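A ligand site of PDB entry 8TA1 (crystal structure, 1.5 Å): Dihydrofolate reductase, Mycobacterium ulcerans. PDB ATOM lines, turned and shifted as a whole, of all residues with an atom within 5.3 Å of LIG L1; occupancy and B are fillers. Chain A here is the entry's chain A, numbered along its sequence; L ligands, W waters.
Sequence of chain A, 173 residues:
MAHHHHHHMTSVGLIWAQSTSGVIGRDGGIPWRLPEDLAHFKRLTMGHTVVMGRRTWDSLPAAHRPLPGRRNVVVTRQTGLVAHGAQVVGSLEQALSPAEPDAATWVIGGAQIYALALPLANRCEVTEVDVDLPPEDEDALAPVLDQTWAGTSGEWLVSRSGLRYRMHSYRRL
N of Thr 127 lies within hydrogen-bond range of O of Trp 16 (2.9 Å).
The guanidinium group (NH1) of Arg 70 sits at hydrogen-bond distance from the side-chain hydroxyl (OG1) of Thr 45 (3.1 Å).
The side-chain hydroxyl of Tyr 114 lies within hydrogen-bond range of the backbone carbonyl oxygen of Ile 108.
The backbone NH of Trp 16 lies within hydrogen-bond range of the backbone carbonyl oxygen of Glu 125 (3.1 Å).
The side-chain carboxylate (OD1) of Asp 37 is in hydrogen-bond range of the side-chain hydroxyl (OG1) of Thr 127 (2.7 Å).
The backbone NH (N) of Ile 15 sits at hydrogen-bond distance from the backbone carbonyl oxygen (O) of Val 107, at 3.1 Å.
O of Pro 68 lies within hydrogen-bond range of NE of Arg 70.
The backbone carbonyl oxygen (O) of Phe 41 is in hydrogen-bond range of the side-chain hydroxyl (OG1) of Thr 45, 2.8 Å away.
Water W1 lies within hydrogen-bond range of the side-chain hydroxyl of Thr 127, the backbone carbonyl oxygen of Glu 125, a nitrogen (N3) of LIG L1, a ring nitrogen (NE2) of His 40 and the backbone carbonyl oxygen of Trp 16.
O of Ile 15 sits at hydrogen-bond distance from N1 of LIG L1, 2.8 Å away.
An oxygen (O2) of LG2 L2 sits at hydrogen-bond distance from the backbone NH (N) of Thr 56 (3.0 Å).
N of Trp 16 sits close to N2 of LIG L1 (3.5 Å).
A ring nitrogen (ND1) of His 64 lies within hydrogen-bond range of an oxygen (O2) of LIG L1, at 2.6 Å.
The side-chain hydroxyl of Tyr 114 is in hydrogen-bond range of a nitrogen (N1) of LIG L1 (3.3 Å).
NH1 of Arg 70 lies within salt-bridge range of O1 of LIG L1 (2.7 Å).
A nitrogen (N1) of LIG L1 is in hydrogen-bond range of the backbone carbonyl oxygen (O) of Ile 108, 3.0 Å away.
The side-chain hydroxyl of Thr 56 sits at hydrogen-bond distance from an oxygen (O2) of LG2 L2 (2.6 Å).
A nitrogen (N4) of LIG L1 is in hydrogen-bond range of the side-chain carboxylate (OD2) of Asp 37, at 2.7 Å.
Residues that only touch LIG L1: Phe 41, Lys 42, Leu 67, Pro 61, Leu 60, Leu 38, Ala 17, Thr 127 and Ile 30.
Hydrophobic or aromatic side chains that line LIG L1: Ile 15, Ala 17, Ile 30, Leu 38, Phe 41, Leu 60, Pro 61, His 64, Leu 67 and Ile 108.
Of the 25 residues printed, 16 come within 4 Å of LIG L1.
The nearest printed residue that does not touch LIG L1 is Pro 68 (4.02 Å).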
ATOM      1  N   ILE A  15      29.179 -15.662  -2.339  1.00  0.00           N
ATOM      2  CA  ILE A  15      28.824 -14.784  -1.231  1.00  0.00           C
ATOM      3  C   ILE A  15      29.096 -15.559   0.050  1.00  0.00           C
ATOM      4  O   ILE A  15      28.686 -16.725   0.163  1.00  0.00           O
ATOM      5  CB  ILE A  15      27.368 -14.269  -1.345  1.00  0.00           C
ATOM      6  CG1 ILE A  15      27.049 -13.341  -0.185  1.00  0.00           C
ATOM      7  CG2 ILE A  15      26.380 -15.409  -1.466  1.00  0.00           C
ATOM      8  CD1 ILE A  15      25.762 -12.539  -0.407  1.00  0.00           C
ATOM      9  N   TRP A  16      29.851 -14.951   0.956  1.00  0.00           N
ATOM     10  CA  TRP A  16      30.138 -15.561   2.245  1.00  0.00           C
ATOM     11  C   TRP A  16      30.397 -14.485   3.290  1.00  0.00           C
ATOM     12  O   TRP A  16      30.683 -13.326   2.973  1.00  0.00           O
ATOM     13  CB  TRP A  16      31.337 -16.518   2.203  1.00  0.00           C
ATOM     14  CG  TRP A  16      32.729 -15.939   2.100  1.00  0.00           C
ATOM     15  CD1 TRP A  16      33.544 -15.541   3.137  1.00  0.00           C
ATOM     16  CD2 TRP A  16      33.502 -15.767   0.909  1.00  0.00           C
ATOM     17  NE1 TRP A  16      34.764 -15.141   2.653  1.00  0.00           N
ATOM     18  CE2 TRP A  16      34.776 -15.283   1.287  1.00  0.00           C
ATOM     19  CE3 TRP A  16      33.249 -16.002  -0.458  1.00  0.00           C
ATOM     20  CZ2 TRP A  16      35.772 -14.984   0.358  1.00  0.00           C
ATOM     21  CZ3 TRP A  16      34.244 -15.705  -1.377  1.00  0.00           C
ATOM     22  CH2 TRP A  16      35.494 -15.214  -0.962  1.00  0.00           C
ATOM     23  N   ALA A  17      30.280 -14.894   4.554  1.00  0.00           N
ATOM     24  CA  ALA A  17      30.653 -14.096   5.732  1.00  0.00           C
ATOM     25  C   ALA A  17      31.747 -14.854   6.486  1.00  0.00           C
ATOM     26  O   ALA A  17      31.596 -16.047   6.761  1.00  0.00           O
ATOM     27  CB  ALA A  17      29.444 -13.913   6.612  1.00  0.00           C
ATOM     28  N   ILE A  30      27.076 -21.294  12.204  1.00  0.00           N
ATOM     29  CA  ILE A  30      27.828 -20.048  12.052  1.00  0.00           C
ATOM     30  C   ILE A  30      28.142 -19.564  13.465  1.00  0.00           C
ATOM     31  O   ILE A  30      27.221 -19.328  14.244  1.00  0.00           O
ATOM     32  CB  ILE A  30      27.004 -18.962  11.344  1.00  0.00           C
ATOM     33  CG1 ILE A  30      26.307 -19.514  10.087  1.00  0.00           C
ATOM     34  CG2 ILE A  30      27.910 -17.762  11.030  1.00  0.00           C
ATOM     35  CD1 ILE A  30      27.238 -19.805   9.018  1.00  0.00           C
ATOM     36  N   LEU A  34      25.139 -11.973  13.392  1.00  0.00           N
ATOM     37  CA  LEU A  34      25.272 -10.682  12.718  1.00  0.00           C
ATOM     38  C   LEU A  34      24.035 -10.419  11.870  1.00  0.00           C
ATOM     39  O   LEU A  34      23.978 -10.765  10.677  1.00  0.00           O
ATOM     40  CB  LEU A  34      26.557 -10.627  11.894  1.00  0.00           C
ATOM     41  CG  LEU A  34      26.858  -9.345  11.133  1.00  0.00           C
ATOM     42  CD1 LEU A  34      26.869  -8.139  12.049  1.00  0.00           C
ATOM     43  CD2 LEU A  34      28.185  -9.444  10.372  1.00  0.00           C
ATOM     44  N   ASP A  37      24.233  -8.920   8.397  1.00  0.00           N
ATOM     45  CA  ASP A  37      24.706  -9.789   7.319  1.00  0.00           C
ATOM     46  C   ASP A  37      23.595 -10.676   6.795  1.00  0.00           C
ATOM     47  O   ASP A  37      23.520 -10.916   5.589  1.00  0.00           O
ATOM     48  CB  ASP A  37      25.885 -10.654   7.771  1.00  0.00           C
ATOM     49  CG  ASP A  37      26.285 -11.646   6.699  1.00  0.00           C
ATOM     50  OD1 ASP A  37      26.759 -11.188   5.641  1.00  0.00           O
ATOM     51  OD2 ASP A  37      26.076 -12.873   6.900  1.00  0.00           O
ATOM     52  N   LEU A  38      22.733 -11.191   7.663  1.00  0.00           N
ATOM     53  CA  LEU A  38      21.555 -11.908   7.176  1.00  0.00           C
ATOM     54  C   LEU A  38      20.748 -11.032   6.236  1.00  0.00           C
ATOM     55  O   LEU A  38      20.296 -11.492   5.170  1.00  0.00           O
ATOM     56  CB  LEU A  38      20.711 -12.420   8.342  1.00  0.00           C
ATOM     57  CG  LEU A  38      19.409 -13.179   8.024  1.00  0.00           C
ATOM     58  CD1 LEU A  38      19.062 -14.179   9.152  1.00  0.00           C
ATOM     59  CD2 LEU A  38      18.265 -12.224   7.852  1.00  0.00           C
ATOM     60  N   HIS A  40      21.839  -8.438   4.441  1.00  0.00           N
ATOM     61  CA  HIS A  40      22.643  -8.279   3.224  1.00  0.00           C
ATOM     62  C   HIS A  40      22.527  -9.500   2.330  1.00  0.00           C
ATOM     63  O   HIS A  40      22.367  -9.395   1.103  1.00  0.00           O
ATOM     64  CB  HIS A  40      24.091  -8.075   3.693  1.00  0.00           C
ATOM     65  CG  HIS A  40      25.132  -8.102   2.618  1.00  0.00           C
ATOM     66  ND1 HIS A  40      25.260  -7.126   1.657  1.00  0.00           N
ATOM     67  CD2 HIS A  40      26.174  -8.954   2.438  1.00  0.00           C
ATOM     68  CE1 HIS A  40      26.311  -7.395   0.905  1.00  0.00           C
ATOM     69  NE2 HIS A  40      26.885  -8.497   1.347  1.00  0.00           N
ATOM     70  N   PHE A  41      22.612 -10.691   2.929  1.00  0.00           N
ATOM     71  CA  PHE A  41      22.509 -11.925   2.179  1.00  0.00           C
ATOM     72  C   PHE A  41      21.159 -12.039   1.500  1.00  0.00           C
ATOM     73  O   PHE A  41      21.065 -12.328   0.306  1.00  0.00           O
ATOM     74  CB  PHE A  41      22.767 -13.117   3.121  1.00  0.00           C
ATOM     75  CG  PHE A  41      22.584 -14.450   2.460  1.00  0.00           C
ATOM     76  CD1 PHE A  41      23.540 -14.937   1.600  1.00  0.00           C
ATOM     77  CD2 PHE A  41      21.446 -15.210   2.688  1.00  0.00           C
ATOM     78  CE1 PHE A  41      23.372 -16.158   0.983  1.00  0.00           C
ATOM     79  CE2 PHE A  41      21.261 -16.443   2.057  1.00  0.00           C
ATOM     80  CZ  PHE A  41      22.226 -16.913   1.211  1.00  0.00           C
ATOM     81  N   LYS A  42      20.072 -11.794   2.243  1.00  0.00           N
ATOM     82  CA  LYS A  42      18.745 -11.817   1.628  1.00  0.00           C
ATOM     83  C   LYS A  42      18.633 -10.781   0.521  1.00  0.00           C
ATOM     84  O   LYS A  42      18.081 -11.076  -0.555  1.00  0.00           O
ATOM     85  CB  LYS A  42      17.661 -11.536   2.660  1.00  0.00           C
ATOM     86  CG  LYS A  42      17.375 -12.668   3.570  1.00  0.00           C
ATOM     87  CD  LYS A  42      16.146 -12.349   4.410  1.00  0.00           C
ATOM     88  CE  LYS A  42      15.673 -13.547   5.181  1.00  0.00           C
ATOM     89  NZ  LYS A  42      14.442 -13.219   5.981  1.00  0.00           N
ATOM     90  N   THR A  45      20.398 -12.023  -2.643  1.00  0.00           N
ATOM     91  CA  THR A  45      19.996 -13.295  -3.211  1.00  0.00           C
ATOM     92  C   THR A  45      18.507 -13.407  -3.546  1.00  0.00           C
ATOM     93  O   THR A  45      18.147 -14.290  -4.324  1.00  0.00           O
ATOM     94  CB  THR A  45      20.395 -14.498  -2.329  1.00  0.00           C
ATOM     95  OG1 THR A  45      19.772 -14.436  -1.040  1.00  0.00           O
ATOM     96  CG2 THR A  45      21.912 -14.625  -2.166  1.00  0.00           C
ATOM     97  N   THR A  56      25.805 -27.513   3.867  1.00  0.00           N
ATOM     98  CA  THR A  56      25.162 -26.217   4.075  1.00  0.00           C
ATOM     99  C   THR A  56      23.632 -26.364   4.045  1.00  0.00           C
ATOM    100  O   THR A  56      22.944 -25.798   4.906  1.00  0.00           O
ATOM    101  CB  THR A  56      25.667 -25.210   3.045  1.00  0.00           C
ATOM    102  OG1 THR A  56      27.040 -24.918   3.277  1.00  0.00           O
ATOM    103  CG2 THR A  56      24.903 -23.897   3.163  1.00  0.00           C
ATOM    104  N   SER A  59      22.618 -27.490   7.271  1.00  0.00           N
ATOM    105  CA  SER A  59      22.869 -26.490   8.306  1.00  0.00           C
ATOM    106  C   SER A  59      21.768 -25.436   8.405  1.00  0.00           C
ATOM    107  O   SER A  59      21.742 -24.675   9.382  1.00  0.00           O
ATOM    108  CB  SER A  59      24.214 -25.776   8.067  1.00  0.00           C
ATOM    109  OG  SER A  59      24.146 -24.765   7.077  1.00  0.00           O
ATOM    110  N   LEU A  60      20.856 -25.372   7.438  1.00  0.00           N
ATOM    111  CA  LEU A  60      19.912 -24.275   7.393  1.00  0.00           C
ATOM    112  C   LEU A  60      18.875 -24.411   8.514  1.00  0.00           C
ATOM    113  O   LEU A  60      18.337 -25.499   8.726  1.00  0.00           O
ATOM    114  CB  LEU A  60      19.213 -24.234   6.042  1.00  0.00           C
ATOM    115  CG  LEU A  60      20.088 -23.895   4.833  1.00  0.00           C
ATOM    116  CD1 LEU A  60      19.272 -24.017   3.579  1.00  0.00           C
ATOM    117  CD2 LEU A  60      20.673 -22.490   4.956  1.00  0.00           C
ATOM    118  N   PRO A  61      18.560 -23.339   9.221  1.00  0.00           N
ATOM    119  CA  PRO A  61      17.519 -23.420  10.244  1.00  0.00           C
ATOM    120  C   PRO A  61      16.167 -23.728   9.607  1.00  0.00           C
ATOM    121  O   PRO A  61      15.943 -23.466   8.426  1.00  0.00           O
ATOM    122  CB  PRO A  61      17.528 -22.014  10.864  1.00  0.00           C
ATOM    123  CG  PRO A  61      18.837 -21.453  10.552  1.00  0.00           C
ATOM    124  CD  PRO A  61      19.246 -22.040   9.227  1.00  0.00           C
ATOM    125  N   HIS A  64      14.238 -21.625   7.252  1.00  0.00           N
ATOM    126  CA  HIS A  64      15.052 -21.196   6.124  1.00  0.00           C
ATOM    127  C   HIS A  64      15.519 -22.372   5.269  1.00  0.00           C
ATOM    128  O   HIS A  64      16.454 -22.231   4.488  1.00  0.00           O
ATOM    129  CB  HIS A  64      16.238 -20.368   6.613  1.00  0.00           C
ATOM    130  CG  HIS A  64      15.814 -19.153   7.387  1.00  0.00           C
ATOM    131  ND1 HIS A  64      15.728 -17.899   6.825  1.00  0.00           N
ATOM    132  CD2 HIS A  64      15.410 -19.018   8.678  1.00  0.00           C
ATOM    133  CE1 HIS A  64      15.298 -17.045   7.736  1.00  0.00           C
ATOM    134  NE2 HIS A  64      15.089 -17.693   8.869  1.00  0.00           N
ATOM    135  N   LEU A  67      15.521 -21.864   1.522  1.00  0.00           N
ATOM    136  CA  LEU A  67      15.640 -20.417   1.655  1.00  0.00           C
ATOM    137  C   LEU A  67      14.487 -19.755   0.912  1.00  0.00           C
ATOM    138  O   LEU A  67      14.396 -19.910  -0.320  1.00  0.00           O
ATOM    139  CB  LEU A  67      16.980 -19.944   1.105  1.00  0.00           C
ATOM    140  CG  LEU A  67      18.186 -20.453   1.872  1.00  0.00           C
ATOM    141  CD1 LEU A  67      19.420 -20.372   1.002  1.00  0.00           C
ATOM    142  CD2 LEU A  67      18.366 -19.673   3.109  1.00  0.00           C
ATOM    143  N   PRO A  68      13.582 -19.055   1.598  1.00  0.00           N
ATOM    144  CA  PRO A  68      12.353 -18.608   0.923  1.00  0.00           C
ATOM    145  C   PRO A  68      12.635 -17.544  -0.107  1.00  0.00           C
ATOM    146  O   PRO A  68      13.438 -16.642   0.103  1.00  0.00           O
ATOM    147  CB  PRO A  68      11.502 -18.051   2.071  1.00  0.00           C
ATOM    148  CG  PRO A  68      12.443 -17.784   3.177  1.00  0.00           C
ATOM    149  CD  PRO A  68      13.543 -18.807   3.041  1.00  0.00           C
ATOM    150  N   ARG A  70      13.921 -17.942  -3.073  1.00  0.00           N
ATOM    151  CA  ARG A  70      15.093 -18.213  -3.876  1.00  0.00           C
ATOM    152  C   ARG A  70      14.978 -19.613  -4.451  1.00  0.00           C
ATOM    153  O   ARG A  70      14.306 -20.471  -3.881  1.00  0.00           O
ATOM    154  CB  ARG A  70      16.318 -18.061  -3.020  1.00  0.00           C
ATOM    155  CG  ARG A  70      16.593 -16.581  -2.849  1.00  0.00           C
ATOM    156  CD  ARG A  70      17.177 -16.215  -1.567  1.00  0.00           C
ATOM    157  NE  ARG A  70      16.266 -16.333  -0.434  1.00  0.00           N
ATOM    158  CZ  ARG A  70      16.702 -16.204   0.820  1.00  0.00           C
ATOM    159  NH1 ARG A  70      17.947 -15.867   1.076  1.00  0.00           N
ATOM    160  NH2 ARG A  70      15.844 -16.395   1.812  1.00  0.00           N
ATOM    161  N   VAL A 107      26.687 -18.739  -5.411  1.00  0.00           N
ATOM    162  CA  VAL A 107      27.180 -19.886  -4.671  1.00  0.00           C
ATOM    163  C   VAL A 107      27.297 -19.451  -3.214  1.00  0.00           C
ATOM    164  O   VAL A 107      27.998 -18.487  -2.903  1.00  0.00           O
ATOM    165  CB  VAL A 107      28.512 -20.376  -5.236  1.00  0.00           C
ATOM    166  CG1 VAL A 107      29.106 -21.445  -4.349  1.00  0.00           C
ATOM    167  CG2 VAL A 107      28.304 -20.897  -6.645  1.00  0.00           C
ATOM    168  N   ILE A 108      26.551 -20.105  -2.331  1.00  0.00           N
ATOM    169  CA  ILE A 108      26.350 -19.632  -0.974  1.00  0.00           C
ATOM    170  C   ILE A 108      27.039 -20.516   0.059  1.00  0.00           C
ATOM    171  O   ILE A 108      26.787 -20.356   1.255  1.00  0.00           O
ATOM    172  CB  ILE A 108      24.844 -19.441  -0.650  1.00  0.00           C
ATOM    173  CG1 ILE A 108      24.105 -20.786  -0.629  1.00  0.00           C
ATOM    174  CG2 ILE A 108      24.200 -18.496  -1.648  1.00  0.00           C
ATOM    175  CD1 ILE A 108      22.803 -20.702   0.135  1.00  0.00           C
ATOM    176  N   GLY A 109      27.883 -21.431  -0.363  1.00  0.00           N
ATOM    177  CA  GLY A 109      28.732 -22.205   0.533  1.00  0.00           C
ATOM    178  C   GLY A 109      28.433 -23.695   0.428  1.00  0.00           C
ATOM    179  O   GLY A 109      27.568 -24.128  -0.335  1.00  0.00           O
ATOM    180  N   TYR A 114      32.800 -23.655  -2.196  1.00  0.00           N
ATOM    181  CA  TYR A 114      33.471 -22.416  -2.616  1.00  0.00           C
ATOM    182  C   TYR A 114      34.728 -22.738  -3.400  1.00  0.00           C
ATOM    183  O   TYR A 114      35.050 -22.047  -4.368  1.00  0.00           O
ATOM    184  CB  TYR A 114      33.856 -21.520  -1.436  1.00  0.00           C
ATOM    185  CG  TYR A 114      32.731 -20.813  -0.735  1.00  0.00           C
ATOM    186  CD1 TYR A 114      31.715 -20.168  -1.436  1.00  0.00           C
ATOM    187  CD2 TYR A 114      32.670 -20.811   0.650  1.00  0.00           C
ATOM    188  CE1 TYR A 114      30.685 -19.523  -0.756  1.00  0.00           C
ATOM    189  CE2 TYR A 114      31.624 -20.191   1.326  1.00  0.00           C
ATOM    190  CZ  TYR A 114      30.641 -19.552   0.618  1.00  0.00           C
ATOM    191  OH  TYR A 114      29.615 -18.958   1.304  1.00  0.00           O
ATOM    192  N   GLU A 125      31.157 -11.510  -2.909  1.00  0.00           N
ATOM    193  CA  GLU A 125      30.598 -10.554  -1.968  1.00  0.00           C
ATOM    194  C   GLU A 125      30.877 -11.098  -0.572  1.00  0.00           C
ATOM    195  O   GLU A 125      30.306 -12.132  -0.177  1.00  0.00           O
ATOM    196  CB  GLU A 125      29.098 -10.351  -2.212  1.00  0.00           C
ATOM    197  CG  GLU A 125      28.798  -9.670  -3.527  1.00  0.00           C
ATOM    198  CD  GLU A 125      29.300  -8.240  -3.589  1.00  0.00           C
ATOM    199  OE1 GLU A 125      29.420  -7.598  -2.549  1.00  0.00           O
ATOM    200  OE2 GLU A 125      29.563  -7.734  -4.697  1.00  0.00           O
ATOM    201  N   THR A 127      31.421 -10.625   3.615  1.00  0.00           N
ATOM    202  CA  THR A 127      31.249  -9.889   4.851  1.00  0.00           C
ATOM    203  C   THR A 127      32.378 -10.303   5.778  1.00  0.00           C
ATOM    204  O   THR A 127      32.622 -11.494   5.964  1.00  0.00           O
ATOM    205  CB  THR A 127      29.915 -10.212   5.518  1.00  0.00           C
ATOM    206  OG1 THR A 127      28.858  -9.890   4.615  1.00  0.00           O
ATOM    207  CG2 THR A 127      29.751  -9.396   6.804  1.00  0.00           C
HETATM  208  C1  LIG L   1      23.991 -18.545   3.667  1.00  0.00           C
HETATM  209  C2  LIG L   1      21.572 -19.073   6.988  1.00  0.00           C
HETATM  210  C3  LIG L   1      22.243 -19.534   8.120  1.00  0.00           C
HETATM  211  C4  LIG L   1      23.245 -20.052   5.524  1.00  0.00           C
HETATM  212  C5  LIG L   1      23.654 -19.993   4.059  1.00  0.00           C
HETATM  213  C6  LIG L   1      17.917 -16.502   4.714  1.00  0.00           C
HETATM  214  C7  LIG L   1      18.693 -16.759   5.996  1.00  0.00           C
HETATM  215  C8  LIG L   1      19.663 -17.868   5.840  1.00  0.00           C
HETATM  216  C9  LIG L   1      20.386 -18.342   7.071  1.00  0.00           C
HETATM  217  C10 LIG L   1      19.885 -18.078   8.339  1.00  0.00           C
HETATM  218  C11 LIG L   1      20.528 -18.541   9.507  1.00  0.00           C
HETATM  219  C12 LIG L   1      21.708 -19.265   9.404  1.00  0.00           C
HETATM  220  C13 LIG L   1      25.688 -16.938   4.113  1.00  0.00           C
HETATM  221  C14 LIG L   1      26.438 -16.578   2.988  1.00  0.00           C
HETATM  222  C15 LIG L   1      26.637 -14.420   3.804  1.00  0.00           C
HETATM  223  C16 LIG L   1      25.447 -15.987   5.105  1.00  0.00           C
HETATM  224  C17 LIG L   1      24.654 -16.256   6.374  1.00  0.00           C
HETATM  225  C18 LIG L   1      25.503 -16.060   7.631  1.00  0.00           C
HETATM  226  C19 LIG L   1      24.672 -16.252   8.912  1.00  0.00           C
HETATM  227  C20 LIG L   1      23.438 -15.387   8.990  1.00  0.00           C
HETATM  228  C21 LIG L   1      22.600 -15.523   7.751  1.00  0.00           C
HETATM  229  C22 LIG L   1      23.400 -15.345   6.454  1.00  0.00           C
HETATM  230  N1  LIG L   1      26.703 -17.487   2.004  1.00  0.00           N
HETATM  231  N2  LIG L   1      26.902 -15.313   2.802  1.00  0.00           N
HETATM  232  N3  LIG L   1      27.098 -13.136   3.650  1.00  0.00           N
HETATM  233  N4  LIG L   1      25.927 -14.712   4.942  1.00  0.00           N
HETATM  234  O1  LIG L   1      18.514 -15.936   3.758  1.00  0.00           O
HETATM  235  O2  LIG L   1      16.704 -16.890   4.631  1.00  0.00           O
HETATM  236  O3  LIG L   1      22.033 -19.326   5.714  1.00  0.00           O
HETATM  237  O4  LIG L   1      25.243 -18.234   4.278  1.00  0.00           O
HETATM  238  P1  LG2 L   2      29.546 -27.840   2.041  1.00  0.00           P
HETATM  239  O1  LG2 L   2      30.546 -27.326   1.074  1.00  0.00           O
HETATM  240  O2  LG2 L   2      28.318 -27.028   2.319  1.00  0.00           O
HETATM  241  O3  LG2 L   2      28.960 -29.302   1.608  1.00  0.00           O
HETATM  242  C1  LG2 L   2      29.853 -30.366   1.332  1.00  0.00           C
HETATM  243  C2  LG2 L   2      29.063 -31.434   0.609  1.00  0.00           C
HETATM  244  O4  LG2 L   2      28.901 -31.058  -0.744  1.00  0.00           O
HETATM  245  C3  LG2 L   2      29.758 -32.808   0.586  1.00  0.00           C
HETATM  246  O5  LG2 L   2      29.620 -33.520   1.786  1.00  0.00           O
HETATM  247  C4  LG2 L   2      29.014 -33.411  -0.623  1.00  0.00           C
HETATM  248  O6  LG2 L   2      27.721 -33.721  -0.274  1.00  0.00           O
HETATM  249  C5  LG2 L   2      28.934 -32.192  -1.564  1.00  0.00           C
HETATM  250  N1  LG2 L   2      30.048 -32.106  -2.474  1.00  0.00           N
HETATM  251  C6  LG2 L   2      31.303 -31.603  -2.260  1.00  0.00           C
HETATM  252  N2  LG2 L   2      32.052 -31.708  -3.330  1.00  0.00           N
HETATM  253  C7  LG2 L   2      31.264 -32.301  -4.280  1.00  0.00           C
HETATM  254  C8  LG2 L   2      31.432 -32.688  -5.625  1.00  0.00           C
HETATM  255  N3  LG2 L   2      32.583 -32.495  -6.284  1.00  0.00           N
HETATM  256  N4  LG2 L   2      30.408 -33.251  -6.275  1.00  0.00           N
HETATM  257  C9  LG2 L   2      29.259 -33.443  -5.626  1.00  0.00           C
HETATM  258  N5  LG2 L   2      28.970 -33.120  -4.378  1.00  0.00           N
HETATM  259  C10 LG2 L   2      30.005 -32.545  -3.766  1.00  0.00           C
HETATM  260  O7  LG2 L   2      30.240 -28.252   3.457  1.00  0.00           O
HETATM  261  P2  LG2 L   2      31.293 -27.485   4.417  1.00  0.00           P
HETATM  262  O8  LG2 L   2      32.480 -27.034   3.647  1.00  0.00           O
HETATM  263  O9  LG2 L   2      31.446 -28.403   5.583  1.00  0.00           O
HETATM  264  O10 LG2 L   2      30.491 -26.157   4.876  1.00  0.00           O
HETATM  265  C11 LG2 L   2      29.476 -26.185   5.849  1.00  0.00           C
HETATM  266  C12 LG2 L   2      29.803 -25.250   7.002  1.00  0.00           C
HETATM  267  O11 LG2 L   2      29.915 -23.914   6.461  1.00  0.00           O
HETATM  268  C13 LG2 L   2      28.731 -25.181   8.066  1.00  0.00           C
HETATM  269  O12 LG2 L   2      29.340 -24.841   9.288  1.00  0.00           O
HETATM  270  C14 LG2 L   2      27.894 -23.989   7.631  1.00  0.00           C
HETATM  271  O13 LG2 L   2      27.190 -23.378   8.676  1.00  0.00           O
HETATM  272  C15 LG2 L   2      29.005 -23.088   7.117  1.00  0.00           C
HETATM  273  N6  LG2 L   2      28.626 -22.023   6.163  1.00  0.00           N
HETATM  274  C16 LG2 L   2      28.982 -20.751   6.388  1.00  0.00           C
HETATM  275  C17 LG2 L   2      28.706 -19.757   5.495  1.00  0.00           C
HETATM  276  C18 LG2 L   2      29.124 -18.379   5.832  1.00  0.00           C
HETATM  277  O14 LG2 L   2      29.542 -18.028   6.953  1.00  0.00           O
HETATM  278  N7  LG2 L   2      29.030 -17.572   4.828  1.00  0.00           N
HETATM  279  C19 LG2 L   2      28.008 -20.079   4.322  1.00  0.00           C
HETATM  280  C20 LG2 L   2      27.658 -21.422   4.091  1.00  0.00           C
HETATM  281  C21 LG2 L   2      27.999 -22.379   5.018  1.00  0.00           C
HETATM  282  P3  LG2 L   2      27.358 -35.324   0.159  1.00  0.00           P
HETATM  283  O15 LG2 L   2      25.848 -35.280   0.346  1.00  0.00           O
HETATM  284  O16 LG2 L   2      27.803 -36.180  -1.024  1.00  0.00           O
HETATM  285  O17 LG2 L   2      28.145 -35.623   1.439  1.00  0.00           O
HETATM  286  O   HOH W   1      28.590 -11.049   1.962  1.00  0.00           O
HETATM  287  O   HOH W   2      25.337 -14.528  11.879  1.00  0.00           O
